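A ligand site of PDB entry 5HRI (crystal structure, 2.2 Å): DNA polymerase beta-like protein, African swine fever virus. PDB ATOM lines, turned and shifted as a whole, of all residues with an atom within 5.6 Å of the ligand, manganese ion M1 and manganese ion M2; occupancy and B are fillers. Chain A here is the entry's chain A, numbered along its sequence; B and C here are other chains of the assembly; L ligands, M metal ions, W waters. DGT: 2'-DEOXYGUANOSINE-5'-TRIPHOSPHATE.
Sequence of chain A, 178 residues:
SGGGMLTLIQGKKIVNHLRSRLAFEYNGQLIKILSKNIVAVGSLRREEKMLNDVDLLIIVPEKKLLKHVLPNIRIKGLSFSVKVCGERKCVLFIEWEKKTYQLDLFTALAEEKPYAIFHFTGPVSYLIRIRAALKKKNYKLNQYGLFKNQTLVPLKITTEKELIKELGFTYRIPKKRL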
ATOM      1  N   GLY A  42      30.629  25.785  24.582  1.00  0.00           N
ATOM      2  CA  GLY A  42      30.141  27.139  24.777  1.00  0.00           C
ATOM      3  C   GLY A  42      30.649  28.097  23.721  1.00  0.00           C
ATOM      4  O   GLY A  42      30.962  27.709  22.591  1.00  0.00           O
ATOM      5  N   SER A  43      30.757  29.357  24.113  1.00  0.00           N
ATOM      6  CA  SER A  43      31.061  30.432  23.187  1.00  0.00           C
ATOM      7  C   SER A  43      32.462  30.287  22.632  1.00  0.00           C
ATOM      8  O   SER A  43      32.745  30.802  21.550  1.00  0.00           O
ATOM      9  CB  SER A  43      30.878  31.818  23.843  1.00  0.00           C
ATOM     10  OG  SER A  43      31.479  31.866  25.118  1.00  0.00           O
ATOM     11  N   LEU A  44      33.324  29.573  23.350  1.00  0.00           N
ATOM     12  CA  LEU A  44      34.675  29.332  22.868  1.00  0.00           C
ATOM     13  C   LEU A  44      34.600  28.493  21.597  1.00  0.00           C
ATOM     14  O   LEU A  44      35.176  28.867  20.577  1.00  0.00           O
ATOM     15  CB  LEU A  44      35.522  28.625  23.939  1.00  0.00           C
ATOM     16  CG  LEU A  44      37.056  28.781  23.830  1.00  0.00           C
ATOM     17  CD1 LEU A  44      37.715  28.225  25.076  1.00  0.00           C
ATOM     18  CD2 LEU A  44      37.634  28.089  22.613  1.00  0.00           C
ATOM     19  N   ARG A  46      32.112  28.208  19.651  1.00  0.00           N
ATOM     20  CA  ARG A  46      31.463  29.048  18.652  1.00  0.00           C
ATOM     21  C   ARG A  46      32.314  30.243  18.178  1.00  0.00           C
ATOM     22  O   ARG A  46      31.859  31.021  17.354  1.00  0.00           O
ATOM     23  CB  ARG A  46      30.110  29.556  19.181  1.00  0.00           C
ATOM     24  CG  ARG A  46      29.160  28.435  19.560  1.00  0.00           C
ATOM     25  CD  ARG A  46      27.723  28.929  19.614  1.00  0.00           C
ATOM     26  NE  ARG A  46      27.603  30.176  20.368  1.00  0.00           N
ATOM     27  CZ  ARG A  46      27.479  30.272  21.692  1.00  0.00           C
ATOM     28  NH1 ARG A  46      27.446  29.197  22.467  1.00  0.00           N
ATOM     29  NH2 ARG A  46      27.382  31.468  22.244  1.00  0.00           N
ATOM     30  N   GLU A  48      33.248  33.133  19.401  1.00  0.00           N
ATOM     31  CA  GLU A  48      32.876  34.520  19.691  1.00  0.00           C
ATOM     32  C   GLU A  48      34.128  35.265  20.166  1.00  0.00           C
ATOM     33  O   GLU A  48      34.999  34.681  20.828  1.00  0.00           O
ATOM     34  CB  GLU A  48      31.711  34.598  20.682  1.00  0.00           C
ATOM     35  CG  GLU A  48      30.386  34.839  19.972  1.00  0.00           C
ATOM     36  CD  GLU A  48      29.175  34.464  20.785  1.00  0.00           C
ATOM     37  OE1 GLU A  48      28.164  34.068  20.171  1.00  0.00           O
ATOM     38  OE2 GLU A  48      29.232  34.557  22.041  1.00  0.00           O
ATOM     39  N   MET A  50      34.624  37.728  22.240  1.00  0.00           N
ATOM     40  CA  MET A  50      34.693  37.896  23.688  1.00  0.00           C
ATOM     41  C   MET A  50      33.855  36.824  24.378  1.00  0.00           C
ATOM     42  O   MET A  50      32.729  36.549  23.971  1.00  0.00           O
ATOM     43  CB  MET A  50      34.146  39.251  24.108  1.00  0.00           C
ATOM     44  CG  MET A  50      34.918  40.449  23.556  1.00  0.00           C
ATOM     45  SD  MET A  50      36.679  40.407  23.939  1.00  0.00           S
ATOM     46  CE  MET A  50      36.656  40.514  25.731  1.00  0.00           C
ATOM     47  N   LEU A  51      34.421  36.257  25.440  1.00  0.00           N
ATOM     48  CA  LEU A  51      33.796  35.181  26.188  1.00  0.00           C
ATOM     49  C   LEU A  51      33.541  35.660  27.608  1.00  0.00           C
ATOM     50  O   LEU A  51      34.346  36.413  28.155  1.00  0.00           O
ATOM     51  CB  LEU A  51      34.732  33.973  26.224  1.00  0.00           C
ATOM     52  CG  LEU A  51      35.361  33.538  24.896  1.00  0.00           C
ATOM     53  CD1 LEU A  51      36.547  32.627  25.157  1.00  0.00           C
ATOM     54  CD2 LEU A  51      34.351  32.833  23.997  1.00  0.00           C
ATOM     55  N   ASN A  52      32.429  35.241  28.208  1.00  0.00           N
ATOM     56  CA  ASN A  52      32.185  35.517  29.643  1.00  0.00           C
ATOM     57  C   ASN A  52      32.849  34.498  30.552  1.00  0.00           C
ATOM     58  O   ASN A  52      33.020  34.748  31.744  1.00  0.00           O
ATOM     59  CB  ASN A  52      30.704  35.575  29.986  1.00  0.00           C
ATOM     60  CG  ASN A  52      30.075  36.889  29.585  1.00  0.00           C
ATOM     61  OD1 ASN A  52      30.518  37.955  30.012  1.00  0.00           O
ATOM     62  ND2 ASN A  52      29.039  36.823  28.768  1.00  0.00           N
ATOM     63  N   ASP A  53      33.188  33.344  29.993  1.00  0.00           N
ATOM     64  CA  ASP A  53      33.821  32.277  30.752  1.00  0.00           C
ATOM     65  C   ASP A  53      34.380  31.252  29.795  1.00  0.00           C
ATOM     66  O   ASP A  53      34.261  31.420  28.580  1.00  0.00           O
ATOM     67  CB  ASP A  53      32.802  31.628  31.708  1.00  0.00           C
ATOM     68  CG  ASP A  53      31.538  31.139  31.002  1.00  0.00           C
ATOM     69  OD1 ASP A  53      31.610  30.456  29.955  1.00  0.00           O
ATOM     70  OD2 ASP A  53      30.448  31.418  31.525  1.00  0.00           O
ATOM     71  N   VAL A  54      35.012  30.226  30.344  1.00  0.00           N
ATOM     72  CA  VAL A  54      35.487  29.092  29.569  1.00  0.00           C
ATOM     73  C   VAL A  54      34.669  27.868  29.927  1.00  0.00           C
ATOM     74  O   VAL A  54      34.471  27.567  31.108  1.00  0.00           O
ATOM     75  CB  VAL A  54      36.965  28.784  29.843  1.00  0.00           C
ATOM     76  CG1 VAL A  54      37.395  27.514  29.120  1.00  0.00           C
ATOM     77  CG2 VAL A  54      37.826  29.959  29.379  1.00  0.00           C
ATOM     78  N   ASP A  55      34.209  27.151  28.912  1.00  0.00           N
ATOM     79  CA  ASP A  55      33.303  26.015  29.087  1.00  0.00           C
ATOM     80  C   ASP A  55      33.936  24.741  28.530  1.00  0.00           C
ATOM     81  O   ASP A  55      34.211  24.662  27.340  1.00  0.00           O
ATOM     82  CB  ASP A  55      31.990  26.305  28.351  1.00  0.00           C
ATOM     83  CG  ASP A  55      31.164  27.396  29.007  1.00  0.00           C
ATOM     84  OD1 ASP A  55      30.838  27.266  30.205  1.00  0.00           O
ATOM     85  OD2 ASP A  55      30.796  28.375  28.321  1.00  0.00           O
ATOM     86  N   GLN A 102      36.169  32.696  35.193  1.00  0.00           N
ATOM     87  CA  GLN A 102      35.251  31.591  35.455  1.00  0.00           C
ATOM     88  C   GLN A 102      35.455  30.435  34.476  1.00  0.00           C
ATOM     89  O   GLN A 102      35.368  30.634  33.265  1.00  0.00           O
ATOM     90  CB  GLN A 102      33.811  32.065  35.408  1.00  0.00           C
ATOM     91  CG  GLN A 102      32.804  30.995  35.806  1.00  0.00           C
ATOM     92  CD  GLN A 102      31.394  31.549  35.914  1.00  0.00           C
ATOM     93  OE1 GLN A 102      31.152  32.492  36.642  1.00  0.00           O
ATOM     94  NE2 GLN A 102      30.449  30.938  35.190  1.00  0.00           N
ATOM     95  N   ASP A 104      33.944  26.633  33.571  1.00  0.00           N
ATOM     96  CA  ASP A 104      32.792  25.774  33.791  1.00  0.00           C
ATOM     97  C   ASP A 104      33.112  24.385  33.275  1.00  0.00           C
ATOM     98  O   ASP A 104      33.502  24.213  32.121  1.00  0.00           O
ATOM     99  CB  ASP A 104      31.567  26.274  33.002  1.00  0.00           C
ATOM    100  CG  ASP A 104      31.090  27.650  33.445  1.00  0.00           C
ATOM    101  OD1 ASP A 104      31.309  28.032  34.593  1.00  0.00           O
ATOM    102  OD2 ASP A 104      30.464  28.343  32.611  1.00  0.00           O
ATOM    103  N   PHE A 106      31.708  20.375  32.744  1.00  0.00           N
ATOM    104  CA  PHE A 106      30.506  19.532  32.654  1.00  0.00           C
ATOM    105  C   PHE A 106      30.905  18.102  32.324  1.00  0.00           C
ATOM    106  O   PHE A 106      31.926  17.895  31.673  1.00  0.00           O
ATOM    107  CB  PHE A 106      29.554  20.057  31.575  1.00  0.00           C
ATOM    108  CG  PHE A 106      29.302  21.544  31.669  1.00  0.00           C
ATOM    109  CD1 PHE A 106      28.323  22.043  32.504  1.00  0.00           C
ATOM    110  CD2 PHE A 106      30.023  22.431  30.893  1.00  0.00           C
ATOM    111  CE1 PHE A 106      28.081  23.403  32.592  1.00  0.00           C
ATOM    112  CE2 PHE A 106      29.782  23.789  30.957  1.00  0.00           C
ATOM    113  CZ  PHE A 106      28.802  24.275  31.798  1.00  0.00           C
ATOM    114  N   HIS A 119      24.367  20.241  23.029  1.00  0.00           N
ATOM    115  CA  HIS A 119      23.717  21.034  24.041  1.00  0.00           C
ATOM    116  C   HIS A 119      24.636  22.143  24.539  1.00  0.00           C
ATOM    117  O   HIS A 119      24.251  23.294  24.548  1.00  0.00           O
ATOM    118  CB  HIS A 119      23.297  20.148  25.207  1.00  0.00           C
ATOM    119  CG  HIS A 119      23.039  20.891  26.489  1.00  0.00           C
ATOM    120  ND1 HIS A 119      21.804  21.425  26.810  1.00  0.00           N
ATOM    121  CD2 HIS A 119      23.847  21.160  27.540  1.00  0.00           C
ATOM    122  CE1 HIS A 119      21.865  21.992  28.002  1.00  0.00           C
ATOM    123  NE2 HIS A 119      23.096  21.843  28.462  1.00  0.00           N
ATOM    124  N   PHE A 120      25.862  21.778  24.909  1.00  0.00           N
ATOM    125  CA  PHE A 120      26.805  22.746  25.493  1.00  0.00           C
ATOM    126  C   PHE A 120      27.468  23.673  24.479  1.00  0.00           C
ATOM    127  O   PHE A 120      28.103  24.670  24.849  1.00  0.00           O
ATOM    128  CB  PHE A 120      27.848  22.005  26.338  1.00  0.00           C
ATOM    129  CG  PHE A 120      27.313  21.461  27.633  1.00  0.00           C
ATOM    130  CD1 PHE A 120      26.855  22.325  28.608  1.00  0.00           C
ATOM    131  CD2 PHE A 120      27.278  20.086  27.875  1.00  0.00           C
ATOM    132  CE1 PHE A 120      26.349  21.837  29.806  1.00  0.00           C
ATOM    133  CE2 PHE A 120      26.785  19.604  29.073  1.00  0.00           C
ATOM    134  CZ  PHE A 120      26.324  20.472  30.039  1.00  0.00           C
ATOM    135  N   THR A 121      27.323  23.379  23.189  1.00  0.00           N
ATOM    136  CA  THR A 121      27.813  24.300  22.167  1.00  0.00           C
ATOM    137  C   THR A 121      26.851  25.464  21.992  1.00  0.00           C
ATOM    138  O   THR A 121      27.276  26.559  21.680  1.00  0.00           O
ATOM    139  CB  THR A 121      28.055  23.581  20.833  1.00  0.00           C
ATOM    140  OG1 THR A 121      29.115  22.641  21.027  1.00  0.00           O
ATOM    141  CG2 THR A 121      28.464  24.556  19.746  1.00  0.00           C
ATOM    142  N   GLY A 122      25.559  25.238  22.187  1.00  0.00           N
ATOM    143  CA  GLY A 122      24.575  26.294  22.025  1.00  0.00           C
ATOM    144  C   GLY A 122      24.565  26.891  20.624  1.00  0.00           C
ATOM    145  O   GLY A 122      24.886  26.200  19.669  1.00  0.00           O
ATOM    146  N   PRO A 123      24.194  28.185  20.501  1.00  0.00           N
ATOM    147  CA  PRO A 123      23.835  29.059  21.623  1.00  0.00           C
ATOM    148  C   PRO A 123      22.471  28.714  22.141  1.00  0.00           C
ATOM    149  O   PRO A 123      21.766  27.903  21.547  1.00  0.00           O
ATOM    150  CB  PRO A 123      23.817  30.459  20.983  1.00  0.00           C
ATOM    151  CG  PRO A 123      23.498  30.206  19.549  1.00  0.00           C
ATOM    152  CD  PRO A 123      24.159  28.888  19.215  1.00  0.00           C
ATOM    153  N   VAL A 124      22.074  29.367  23.227  1.00  0.00           N
ATOM    154  CA  VAL A 124      20.812  29.072  23.875  1.00  0.00           C
ATOM    155  C   VAL A 124      19.636  29.244  22.927  1.00  0.00           C
ATOM    156  O   VAL A 124      18.797  28.361  22.822  1.00  0.00           O
ATOM    157  CB  VAL A 124      20.632  29.939  25.134  1.00  0.00           C
ATOM    158  CG1 VAL A 124      19.236  29.788  25.719  1.00  0.00           C
ATOM    159  CG2 VAL A 124      21.685  29.568  26.174  1.00  0.00           C
ATOM    160  N   LEU A 127      19.172  26.340  20.588  1.00  0.00           N
ATOM    161  CA  LEU A 127      18.683  25.166  21.295  1.00  0.00           C
ATOM    162  C   LEU A 127      17.189  25.224  21.527  1.00  0.00           C
ATOM    163  O   LEU A 127      16.487  24.211  21.376  1.00  0.00           O
ATOM    164  CB  LEU A 127      19.387  25.041  22.651  1.00  0.00           C
ATOM    165  CG  LEU A 127      20.898  24.800  22.568  1.00  0.00           C
ATOM    166  CD1 LEU A 127      21.507  24.722  23.963  1.00  0.00           C
ATOM    167  CD2 LEU A 127      21.224  23.565  21.767  1.00  0.00           C
ATOM    168  N   ARG A 131      14.559  22.559  19.964  1.00  0.00           N
ATOM    169  CA  ARG A 131      13.831  21.719  20.903  1.00  0.00           C
ATOM    170  C   ARG A 131      12.333  21.915  20.810  1.00  0.00           C
ATOM    171  O   ARG A 131      11.569  20.970  21.021  1.00  0.00           O
ATOM    172  CB  ARG A 131      14.318  22.000  22.322  1.00  0.00           C
ATOM    173  CG  ARG A 131      15.709  21.457  22.557  1.00  0.00           C
ATOM    174  CD  ARG A 131      16.304  21.887  23.877  1.00  0.00           C
ATOM    175  NE  ARG A 131      17.599  21.231  24.031  1.00  0.00           N
ATOM    176  CZ  ARG A 131      18.221  21.039  25.185  1.00  0.00           C
ATOM    177  NH1 ARG A 131      17.697  21.436  26.338  1.00  0.00           N
ATOM    178  NH2 ARG A 131      19.395  20.411  25.171  1.00  0.00           N
ATOM    179  P    DA B   9      26.616  29.875  35.686  1.00  0.00           P
ATOM    180  OP1  DA B   9      26.900  29.535  37.103  1.00  0.00           O
ATOM    181  OP2  DA B   9      27.183  31.107  35.076  1.00  0.00           O
ATOM    182  O5'  DA B   9      27.016  28.639  34.771  1.00  0.00           O
ATOM    183  C5'  DA B   9      26.629  28.600  33.389  1.00  0.00           C
ATOM    184  C4'  DA B   9      26.351  27.186  32.953  1.00  0.00           C
ATOM    185  O4'  DA B   9      25.183  26.669  33.639  1.00  0.00           O
ATOM    186  C3'  DA B   9      26.041  27.064  31.462  1.00  0.00           C
ATOM    187  C2'  DA B   9      25.111  25.870  31.410  1.00  0.00           C
ATOM    188  C1'  DA B   9      24.347  25.981  32.718  1.00  0.00           C
ATOM    189  N9   DA B   9      23.077  26.705  32.635  1.00  0.00           N
ATOM    190  C8   DA B   9      22.798  27.987  33.019  1.00  0.00           C
ATOM    191  N7   DA B   9      21.537  28.318  32.850  1.00  0.00           N
ATOM    192  C5   DA B   9      20.954  27.173  32.324  1.00  0.00           C
ATOM    193  C6   DA B   9      19.639  26.878  31.932  1.00  0.00           C
ATOM    194  N6   DA B   9      18.625  27.742  31.997  1.00  0.00           N
ATOM    195  N1   DA B   9      19.394  25.640  31.442  1.00  0.00           N
ATOM    196  C2   DA B   9      20.414  24.766  31.370  1.00  0.00           C
ATOM    197  N3   DA B   9      21.687  24.935  31.715  1.00  0.00           N
ATOM    198  C4   DA B   9      21.899  26.172  32.180  1.00  0.00           C
ATOM    199  P    DC C   9       8.851  26.093  24.812  1.00  0.00           P
ATOM    200  OP1  DC C   9       7.615  25.345  25.134  1.00  0.00           O
ATOM    201  OP2  DC C   9       9.494  26.935  25.841  1.00  0.00           O
ATOM    202  O5'  DC C   9       9.888  25.037  24.234  1.00  0.00           O
ATOM    203  C5'  DC C   9      11.270  25.384  24.045  1.00  0.00           C
ATOM    204  C4'  DC C   9      12.103  24.145  24.225  1.00  0.00           C
ATOM    205  O4'  DC C   9      13.453  24.520  24.575  1.00  0.00           O
ATOM    206  C3'  DC C   9      11.625  23.242  25.344  1.00  0.00           C
ATOM    207  O3'  DC C   9      11.937  21.877  25.059  1.00  0.00           O
ATOM    208  C2'  DC C   9      12.401  23.755  26.544  1.00  0.00           C
ATOM    209  C1'  DC C   9      13.729  24.141  25.918  1.00  0.00           C
ATOM    210  N1   DC C   9      14.398  25.274  26.573  1.00  0.00           N
ATOM    211  C2   DC C   9      15.749  25.158  26.931  1.00  0.00           C
ATOM    212  O2   DC C   9      16.348  24.103  26.661  1.00  0.00           O
ATOM    213  N3   DC C   9      16.361  26.196  27.535  1.00  0.00           N
ATOM    214  C4   DC C   9      15.685  27.320  27.793  1.00  0.00           C
ATOM    215  N4   DC C   9      16.330  28.323  28.393  1.00  0.00           N
ATOM    216  C5   DC C   9      14.314  27.461  27.453  1.00  0.00           C
ATOM    217  C6   DC C   9      13.712  26.433  26.839  1.00  0.00           C
ATOM    218  P    DT C  10      11.351  20.716  25.974  1.00  0.00           P
ATOM    219  OP1  DT C  10      11.244  19.497  25.141  1.00  0.00           O
ATOM    220  OP2  DT C  10      10.163  21.234  26.675  1.00  0.00           O
ATOM    221  O5'  DT C  10      12.504  20.494  27.055  1.00  0.00           O
ATOM    222  C5'  DT C  10      13.813  20.067  26.635  1.00  0.00           C
ATOM    223  C4'  DT C  10      14.775  20.129  27.806  1.00  0.00           C
ATOM    224  O4'  DT C  10      15.148  21.494  28.075  1.00  0.00           O
ATOM    225  C3'  DT C  10      14.237  19.579  29.122  1.00  0.00           C
ATOM    226  O3'  DT C  10      14.840  18.298  29.363  1.00  0.00           O
ATOM    227  C2'  DT C  10      14.632  20.620  30.161  1.00  0.00           C
ATOM    228  C1'  DT C  10      15.593  21.526  29.413  1.00  0.00           C
ATOM    229  N1   DT C  10      15.608  22.939  29.861  1.00  0.00           N
ATOM    230  C2   DT C  10      16.826  23.503  30.180  1.00  0.00           C
ATOM    231  O2   DT C  10      17.886  22.916  30.083  1.00  0.00           O
ATOM    232  N3   DT C  10      16.747  24.817  30.598  1.00  0.00           N
ATOM    233  C4   DT C  10      15.605  25.582  30.737  1.00  0.00           C
ATOM    234  O4   DT C  10      15.704  26.736  31.116  1.00  0.00           O
ATOM    235  C5   DT C  10      14.372  24.922  30.387  1.00  0.00           C
ATOM    236  C7   DT C  10      13.084  25.673  30.506  1.00  0.00           C
ATOM    237  C6   DT C  10      14.430  23.649  29.972  1.00  0.00           C
HETATM  238  PG  DGT L   1      29.110  33.265  27.287  1.00  0.00           P
HETATM  239  O1G DGT L   1      28.181  34.349  27.788  1.00  0.00           O
HETATM  240  O2G DGT L   1      29.522  32.238  28.316  1.00  0.00           O
HETATM  241  O3G DGT L   1      30.279  33.799  26.517  1.00  0.00           O
HETATM  242  O3B DGT L   1      28.266  32.431  26.174  1.00  0.00           O
HETATM  243  PB  DGT L   1      27.974  30.848  26.304  1.00  0.00           P
HETATM  244  O1B DGT L   1      27.236  30.410  25.071  1.00  0.00           O
HETATM  245  O2B DGT L   1      29.307  30.262  26.663  1.00  0.00           O
HETATM  246  O3A DGT L   1      26.952  30.756  27.549  1.00  0.00           O
HETATM  247  PA  DGT L   1      27.081  29.931  28.944  1.00  0.00           P
HETATM  248  O1A DGT L   1      25.979  30.582  29.717  1.00  0.00           O
HETATM  249  O2A DGT L   1      28.528  29.719  29.400  1.00  0.00           O
HETATM  250  O5' DGT L   1      26.474  28.479  28.545  1.00  0.00           O
HETATM  251  C5' DGT L   1      27.339  27.483  28.026  1.00  0.00           C
HETATM  252  C4' DGT L   1      26.493  26.534  27.213  1.00  0.00           C
HETATM  253  O4' DGT L   1      25.556  25.871  28.081  1.00  0.00           O
HETATM  254  C3' DGT L   1      25.624  27.226  26.177  1.00  0.00           C
HETATM  255  O3' DGT L   1      26.332  27.510  24.970  1.00  0.00           O
HETATM  256  C2' DGT L   1      24.482  26.230  26.031  1.00  0.00           C
HETATM  257  C1' DGT L   1      24.312  25.689  27.446  1.00  0.00           C
HETATM  258  N9  DGT L   1      23.248  26.480  28.066  1.00  0.00           N
HETATM  259  C8  DGT L   1      23.399  27.617  28.789  1.00  0.00           C
HETATM  260  N7  DGT L   1      22.207  28.107  29.157  1.00  0.00           N
HETATM  261  C5  DGT L   1      21.273  27.288  28.687  1.00  0.00           C
HETATM  262  C6  DGT L   1      19.813  27.242  28.721  1.00  0.00           C
HETATM  263  O6  DGT L   1      19.160  28.116  29.312  1.00  0.00           O
HETATM  264  N1  DGT L   1      19.216  26.237  28.105  1.00  0.00           N
HETATM  265  C2  DGT L   1      19.897  25.272  27.450  1.00  0.00           C
HETATM  266  N2  DGT L   1      19.210  24.274  26.854  1.00  0.00           N
HETATM  267  N3  DGT L   1      21.244  25.253  27.374  1.00  0.00           N
HETATM  268  C4  DGT L   1      21.966  26.217  27.966  1.00  0.00           C
HETATM  269 MN    MN M   1      30.249  30.341  28.457  1.00  0.00          MN
HETATM  270 MN    MN M   2      29.434  28.591  30.861  1.00  0.00          MN
HETATM  271  O   HOH W   1      22.062  30.539  29.827  1.00  0.00           O
HETATM  272  O   HOH W   2      31.972  30.613  27.151  1.00  0.00           O
HETATM  273  O   HOH W   3      27.790  32.211  30.843  1.00  0.00           O
HETATM  274  O   HOH W   4      30.266  35.862  24.629  1.00  0.00           O
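The backbone NH (N) of Ser 43 lies close to an oxygen (O2B) of the ligand (3.1 Å). ND2 of Asn 52 is in hydrogen-bond range of O1G of the ligand. N1 of DA 9 of chain B sits close to N1 of the ligand (3.4 Å). The backbone carbonyl oxygen (O) of Phe 120 lies within hydrogen-bond range of an oxygen (O3') of the ligand (3.3 Å). An oxygen (O1B) of the ligand is in salt-bridge range of the guanidinium group (NH1) of Arg 46 (2.9 Å). N of Asn 52 sits at hydrogen-bond distance from O3G of the ligand (3.1 Å). O3G of the ligand sits at hydrogen-bond distance from OG of Ser 43. O2 of DC 9 of chain C sits at hydrogen-bond distance from a nitrogen (N2) of the ligand (2.9 Å).
The guanidinium group of Arg 46 is in hydrogen-bond range of the backbone carbonyl oxygen of Thr 121, 2.8 Å away. The side-chain amide nitrogen (NE2) of Gln 102 is in hydrogen-bond range of OP2 of DA 9 of chain B. O2 of DC 9 of chain C sits at hydrogen-bond distance from the guanidinium group of Arg 131, at 3.0 Å. The backbone NH of Asp 104 lies within hydrogen-bond range of the backbone carbonyl oxygen of Val 54 (2.7 Å). O of Ser 43 is in hydrogen-bond range of N of Glu 48 (3.2 Å). A ring nitrogen (ND1) of His 119 sits at hydrogen-bond distance from the guanidinium group (NH2) of Arg 131, 3.1 Å away. NH1 of Arg 131 lies within hydrogen-bond range of O4' of DT 10 of chain C (3.1 Å). The guanidinium group (NH2) of Arg 46 lies within salt-bridge range of the side-chain carboxylate (OE1) of Glu 48, at 3.4 Å.
The guanidinium group (NH1) of Arg 131 lies close to a nitrogen (N2) of the ligand, at 3.3 Å. Residues that only touch the ligand: Gly 42 (3.7 Å), Leu 51 (3.8 Å), His 119 (3.3 Å), Thr 121 (3.6 Å), Gly 122 (3.6 Å), Val 124 (3.4 Å), Leu 127 (3.5 Å) and DT 10 of chain C (3.7 Å). Hydrophobic or aromatic side chains that line the ligand: His 119, Phe 120, Val 124 and Leu 127. The nearest printed residue that does not touch the ligand is Pro 123 (4.5 Å).
Residues that only touch manganese ion M1: Ser 43.
Merely in contact with manganese ion M2: DA 9 of chain B (3.8 Å). Four residues have an atom within 4 Å of manganese ion M2: Asp 53, Asp 55, Asp 104 and DA 9 of chain B. The nearest printed residue that does not touch manganese ion M2 is Phe 106 (4.5 Å).
Manganese ion M1 is bound by O2B of the ligand (2.0 Å). OD1 of Asp 53 is bound to manganese ion M1 (2.0 Å). Manganese ion M1 is bound by O2G of the ligand, at 2.0 Å. OD2 of Asp 55 binds manganese ion M1, at 2.0 Å. O2A of the ligand is bound to manganese ion M1. Manganese ion M1 is bound by water W2, at 2.2 Å.
Manganese ion M2 is bound by the side-chain carboxylate (OD1) of Asp 55, 2.0 Å away. OD2 of Asp 104 binds manganese ion M2, 2.0 Å away. O2A of the ligand is bound to manganese ion M2 (2.1 Å). Manganese ion M2 has three donor atoms within binding distance. Slightly farther from manganese ion M2 lies the side-chain carboxylate (OD2) of Asp 55 (2.9 Å).
Water W2 lies within hydrogen-bond range of the side-chain hydroxyl (OG) of Ser 43 (2.4 Å) and the backbone carbonyl oxygen (O) of Asp 53 (2.8 Å). Water W3 bridges O1A of the ligand and OD2 of Asp 53. Water W4 lies within hydrogen-bond range of O of Met 50, O3G of the ligand and OE2 of Glu 48.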
